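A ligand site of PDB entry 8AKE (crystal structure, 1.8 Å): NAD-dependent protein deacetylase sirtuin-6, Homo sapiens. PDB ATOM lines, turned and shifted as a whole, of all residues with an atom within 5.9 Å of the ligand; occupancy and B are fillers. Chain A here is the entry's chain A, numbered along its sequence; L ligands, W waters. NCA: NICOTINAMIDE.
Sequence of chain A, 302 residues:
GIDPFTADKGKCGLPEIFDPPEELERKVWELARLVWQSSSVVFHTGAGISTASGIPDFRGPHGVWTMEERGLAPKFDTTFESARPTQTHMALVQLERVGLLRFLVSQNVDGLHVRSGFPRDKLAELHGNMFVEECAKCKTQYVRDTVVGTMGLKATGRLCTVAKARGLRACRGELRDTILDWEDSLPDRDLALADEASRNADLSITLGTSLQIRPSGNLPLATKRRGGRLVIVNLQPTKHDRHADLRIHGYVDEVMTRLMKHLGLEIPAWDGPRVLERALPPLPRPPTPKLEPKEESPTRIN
The backbone carbonyl oxygen (O) of Pro 56 sits close to a nitrogen (N1) of the ligand (3.1 Å). Merely in contact with the ligand: Ile 55 (3.6 Å), Phe 58 (3.4 Å), Phe 80 (3.6 Å) and Asn 108 (3.6 Å). Hydrophobic or aromatic side chains that line the ligand: Ile 55, Phe 58, Phe 80 and Val 109. Of the 15 residues printed, 7 come within 4 Å of the ligand. Along chain A the residues within 4 Å of the ligand span positions 55 to 110. The nearest printed residue that does not touch the ligand is Val 64 (4.05 Å).
O7 of the ligand is in hydrogen-bond range of N of Val 109 (3.0 Å). The side-chain carboxylate of Asp 110 lies within hydrogen-bond range of a nitrogen (N7) of the ligand (2.7 Å). An oxygen (O7) of the ligand is in hydrogen-bond range of the backbone NH of Asp 110 (2.9 Å).
The backbone NH (N) of Met 130 lies within hydrogen-bond range of the backbone carbonyl oxygen (O) of Val 109, at 2.8 Å. The backbone carbonyl oxygen (O) of Phe 58 sits at hydrogen-bond distance from the backbone NH (N) of Val 64, 3.3 Å away. The side-chain carboxylate of Asp 110 is in hydrogen-bond range of the side-chain hydroxyl of Ser 50, 3.1 Å away. The backbone NH (N) of Ile 55 sits at hydrogen-bond distance from the backbone carbonyl oxygen (O) of Ser 50 (3.2 Å). The side-chain amide oxygen (OD1) of Asn 108 is in hydrogen-bond range of the backbone NH (N) of Ala 47 (2.9 Å). The side-chain amide nitrogen of Asn 108 sits close to the side-chain carboxylate of Asp 110, at 3.5 Å.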
ATOM      1  N   ALA A  47      26.461  -0.268 -21.076  1.00  0.00           N
ATOM      2  CA  ALA A  47      27.126   0.867 -20.424  1.00  0.00           C
ATOM      3  C   ALA A  47      28.546   0.506 -19.987  1.00  0.00           C
ATOM      4  O   ALA A  47      29.364   1.437 -19.903  1.00  0.00           O
ATOM      5  CB  ALA A  47      26.301   1.382 -19.253  1.00  0.00           C
ATOM      6  N   SER A  50      31.795   1.957 -21.579  1.00  0.00           N
ATOM      7  CA  SER A  50      32.107   3.413 -21.602  1.00  0.00           C
ATOM      8  C   SER A  50      32.529   3.960 -20.227  1.00  0.00           C
ATOM      9  O   SER A  50      32.780   5.231 -20.133  1.00  0.00           O
ATOM     10  CB  SER A  50      30.982   4.157 -22.175  1.00  0.00           C
ATOM     11  OG  SER A  50      30.774   3.679 -23.479  1.00  0.00           O
ATOM     12  N   ILE A  55      32.084   7.718 -18.202  1.00  0.00           N
ATOM     13  CA  ILE A  55      30.603   7.575 -18.159  1.00  0.00           C
ATOM     14  C   ILE A  55      30.232   6.434 -17.224  1.00  0.00           C
ATOM     15  O   ILE A  55      30.575   5.272 -17.454  1.00  0.00           O
ATOM     16  CB  ILE A  55      30.048   7.408 -19.576  1.00  0.00           C
ATOM     17  CG1 ILE A  55      30.457   8.596 -20.442  1.00  0.00           C
ATOM     18  CG2 ILE A  55      28.562   7.211 -19.460  1.00  0.00           C
ATOM     19  CD1 ILE A  55      30.165   8.502 -21.936  1.00  0.00           C
ATOM     20  N   PRO A  56      29.491   6.731 -16.135  1.00  0.00           N
ATOM     21  CA  PRO A  56      29.133   5.689 -15.189  1.00  0.00           C
ATOM     22  C   PRO A  56      28.184   4.746 -15.947  1.00  0.00           C
ATOM     23  O   PRO A  56      27.509   5.214 -16.881  1.00  0.00           O
ATOM     24  CB  PRO A  56      28.511   6.428 -14.003  1.00  0.00           C
ATOM     25  CG  PRO A  56      28.104   7.791 -14.529  1.00  0.00           C
ATOM     26  CD  PRO A  56      28.940   8.050 -15.775  1.00  0.00           C
ATOM     27  N   ASP A  57      28.199   3.463 -15.598  1.00  0.00           N
ATOM     28  CA  ASP A  57      27.144   2.534 -16.060  1.00  0.00           C
ATOM     29  C   ASP A  57      25.854   2.713 -15.257  1.00  0.00           C
ATOM     30  O   ASP A  57      25.710   3.681 -14.481  1.00  0.00           O
ATOM     31  CB  ASP A  57      27.678   1.112 -16.082  1.00  0.00           C
ATOM     32  CG  ASP A  57      28.006   0.463 -14.743  1.00  0.00           C
ATOM     33  OD1 ASP A  57      27.633   0.981 -13.684  1.00  0.00           O
ATOM     34  OD2 ASP A  57      28.672  -0.556 -14.807  1.00  0.00           O
ATOM     35  N   PHE A  58      24.895   1.807 -15.437  1.00  0.00           N
ATOM     36  CA  PHE A  58      23.595   1.878 -14.726  1.00  0.00           C
ATOM     37  C   PHE A  58      23.591   1.001 -13.452  1.00  0.00           C
ATOM     38  O   PHE A  58      23.093   1.465 -12.416  1.00  0.00           O
ATOM     39  CB  PHE A  58      22.479   1.550 -15.747  1.00  0.00           C
ATOM     40  CG  PHE A  58      22.287   2.590 -16.833  1.00  0.00           C
ATOM     41  CD1 PHE A  58      21.496   3.699 -16.626  1.00  0.00           C
ATOM     42  CD2 PHE A  58      22.917   2.462 -18.072  1.00  0.00           C
ATOM     43  CE1 PHE A  58      21.287   4.651 -17.617  1.00  0.00           C
ATOM     44  CE2 PHE A  58      22.719   3.398 -19.070  1.00  0.00           C
ATOM     45  CZ  PHE A  58      21.884   4.489 -18.838  1.00  0.00           C
ATOM     46  N   VAL A  64      24.340   4.466 -12.174  1.00  0.00           N
ATOM     47  CA  VAL A  64      23.290   5.533 -12.106  1.00  0.00           C
ATOM     48  C   VAL A  64      22.171   4.995 -11.201  1.00  0.00           C
ATOM     49  O   VAL A  64      21.954   5.619 -10.149  1.00  0.00           O
ATOM     50  CB  VAL A  64      22.750   5.973 -13.477  1.00  0.00           C
ATOM     51  CG1 VAL A  64      21.548   6.908 -13.370  1.00  0.00           C
ATOM     52  CG2 VAL A  64      23.819   6.633 -14.348  1.00  0.00           C
ATOM     53  N   PHE A  76      30.006  11.540 -13.284  1.00  0.00           N
ATOM     54  CA  PHE A  76      30.571  11.693 -14.668  1.00  0.00           C
ATOM     55  C   PHE A  76      31.936  12.379 -14.545  1.00  0.00           C
ATOM     56  O   PHE A  76      32.039  13.455 -13.888  1.00  0.00           O
ATOM     57  CB  PHE A  76      29.643  12.490 -15.589  1.00  0.00           C
ATOM     58  CG  PHE A  76      28.420  11.766 -16.091  1.00  0.00           C
ATOM     59  CD1 PHE A  76      27.376  11.454 -15.230  1.00  0.00           C
ATOM     60  CD2 PHE A  76      28.284  11.431 -17.436  1.00  0.00           C
ATOM     61  CE1 PHE A  76      26.231  10.826 -15.703  1.00  0.00           C
ATOM     62  CE2 PHE A  76      27.163  10.760 -17.897  1.00  0.00           C
ATOM     63  CZ  PHE A  76      26.140  10.448 -17.030  1.00  0.00           C
ATOM     64  N   PHE A  80      29.277  14.070 -22.329  1.00  0.00           N
ATOM     65  CA  PHE A  80      29.064  13.175 -23.480  1.00  0.00           C
ATOM     66  C   PHE A  80      29.896  13.642 -24.666  1.00  0.00           C
ATOM     67  O   PHE A  80      30.455  12.783 -25.363  1.00  0.00           O
ATOM     68  CB  PHE A  80      27.573  13.059 -23.797  1.00  0.00           C
ATOM     69  CG  PHE A  80      26.823  12.174 -22.835  1.00  0.00           C
ATOM     70  CD1 PHE A  80      27.089  10.814 -22.787  1.00  0.00           C
ATOM     71  CD2 PHE A  80      25.873  12.706 -21.989  1.00  0.00           C
ATOM     72  CE1 PHE A  80      26.409  10.002 -21.892  1.00  0.00           C
ATOM     73  CE2 PHE A  80      25.195  11.905 -21.085  1.00  0.00           C
ATOM     74  CZ  PHE A  80      25.464  10.550 -21.045  1.00  0.00           C
ATOM     75  N   GLN A 107      22.954  -0.811 -26.572  1.00  0.00           N
ATOM     76  CA  GLN A 107      21.943  -0.289 -25.636  1.00  0.00           C
ATOM     77  C   GLN A 107      22.357   1.149 -25.315  1.00  0.00           C
ATOM     78  O   GLN A 107      21.622   1.814 -24.680  1.00  0.00           O
ATOM     79  CB  GLN A 107      21.872  -1.276 -24.483  1.00  0.00           C
ATOM     80  CG  GLN A 107      21.257  -2.626 -24.848  1.00  0.00           C
ATOM     81  CD  GLN A 107      21.191  -3.561 -23.657  1.00  0.00           C
ATOM     82  OE1 GLN A 107      20.364  -3.384 -22.752  1.00  0.00           O
ATOM     83  NE2 GLN A 107      22.046  -4.576 -23.665  1.00  0.00           N
ATOM     84  N   ASN A 108      23.536   1.583 -25.738  1.00  0.00           N
ATOM     85  CA  ASN A 108      24.172   2.800 -25.186  1.00  0.00           C
ATOM     86  C   ASN A 108      23.678   3.983 -26.015  1.00  0.00           C
ATOM     87  O   ASN A 108      23.626   3.885 -27.282  1.00  0.00           O
ATOM     88  CB  ASN A 108      25.696   2.733 -25.228  1.00  0.00           C
ATOM     89  CG  ASN A 108      26.282   1.679 -24.332  1.00  0.00           C
ATOM     90  OD1 ASN A 108      25.630   1.182 -23.407  1.00  0.00           O
ATOM     91  ND2 ASN A 108      27.525   1.339 -24.621  1.00  0.00           N
ATOM     92  N   VAL A 109      23.382   5.068 -25.324  1.00  0.00           N
ATOM     93  CA  VAL A 109      22.875   6.342 -25.928  1.00  0.00           C
ATOM     94  C   VAL A 109      24.056   7.320 -25.988  1.00  0.00           C
ATOM     95  O   VAL A 109      23.853   8.410 -26.526  1.00  0.00           O
ATOM     96  CB  VAL A 109      21.693   6.934 -25.115  1.00  0.00           C
ATOM     97  CG1 VAL A 109      20.407   6.155 -25.258  1.00  0.00           C
ATOM     98  CG2 VAL A 109      22.075   7.149 -23.674  1.00  0.00           C
ATOM     99  N   ASP A 110      25.213   6.945 -25.432  1.00  0.00           N
ATOM    100  CA  ASP A 110      26.413   7.843 -25.253  1.00  0.00           C
ATOM    101  C   ASP A 110      26.994   8.374 -26.590  1.00  0.00           C
ATOM    102  O   ASP A 110      27.952   9.146 -26.518  1.00  0.00           O
ATOM    103  CB  ASP A 110      27.498   7.131 -24.429  1.00  0.00           C
ATOM    104  CG  ASP A 110      28.036   5.830 -25.031  1.00  0.00           C
ATOM    105  OD1 ASP A 110      28.427   5.810 -26.221  1.00  0.00           O
ATOM    106  OD2 ASP A 110      27.999   4.772 -24.323  1.00  0.00           O
ATOM    107  N   GLY A 111      26.530   7.964 -27.765  1.00  0.00           N
ATOM    108  CA  GLY A 111      27.016   8.479 -29.076  1.00  0.00           C
ATOM    109  C   GLY A 111      28.343   7.869 -29.534  1.00  0.00           C
ATOM    110  O   GLY A 111      28.789   8.175 -30.704  1.00  0.00           O
ATOM    111  N   MET A 130      22.217  10.233 -27.906  1.00  0.00           N
ATOM    112  CA  MET A 130      22.148  11.589 -27.337  1.00  0.00           C
ATOM    113  C   MET A 130      22.354  12.625 -28.442  1.00  0.00           C
ATOM    114  O   MET A 130      21.579  13.533 -28.425  1.00  0.00           O
ATOM    115  CB  MET A 130      23.199  11.789 -26.237  1.00  0.00           C
ATOM    116  CG  MET A 130      22.959  10.955 -24.997  1.00  0.00           C
ATOM    117  SD  MET A 130      21.469  11.482 -24.140  1.00  0.00           S
ATOM    118  CE  MET A 130      22.049  12.997 -23.379  1.00  0.00           C
HETATM  119  N1  NCA L   1      24.825   6.077 -18.229  1.00  0.00           N
HETATM  120  C2  NCA L   1      25.367   5.567 -19.348  1.00  0.00           C
HETATM  121  C3  NCA L   1      25.083   6.052 -20.617  1.00  0.00           C
HETATM  122  C4  NCA L   1      24.237   7.151 -20.709  1.00  0.00           C
HETATM  123  C5  NCA L   1      23.645   7.668 -19.573  1.00  0.00           C
HETATM  124  C6  NCA L   1      24.007   7.128 -18.373  1.00  0.00           C
HETATM  125  C7  NCA L   1      25.722   5.489 -21.861  1.00  0.00           C
HETATM  126  O7  NCA L   1      25.099   5.509 -22.925  1.00  0.00           O
HETATM  127  N7  NCA L   1      26.973   5.057 -21.798  1.00  0.00           N
HETATM  128  O   HOH W   1      29.173   3.940 -19.570  1.00  0.00           O
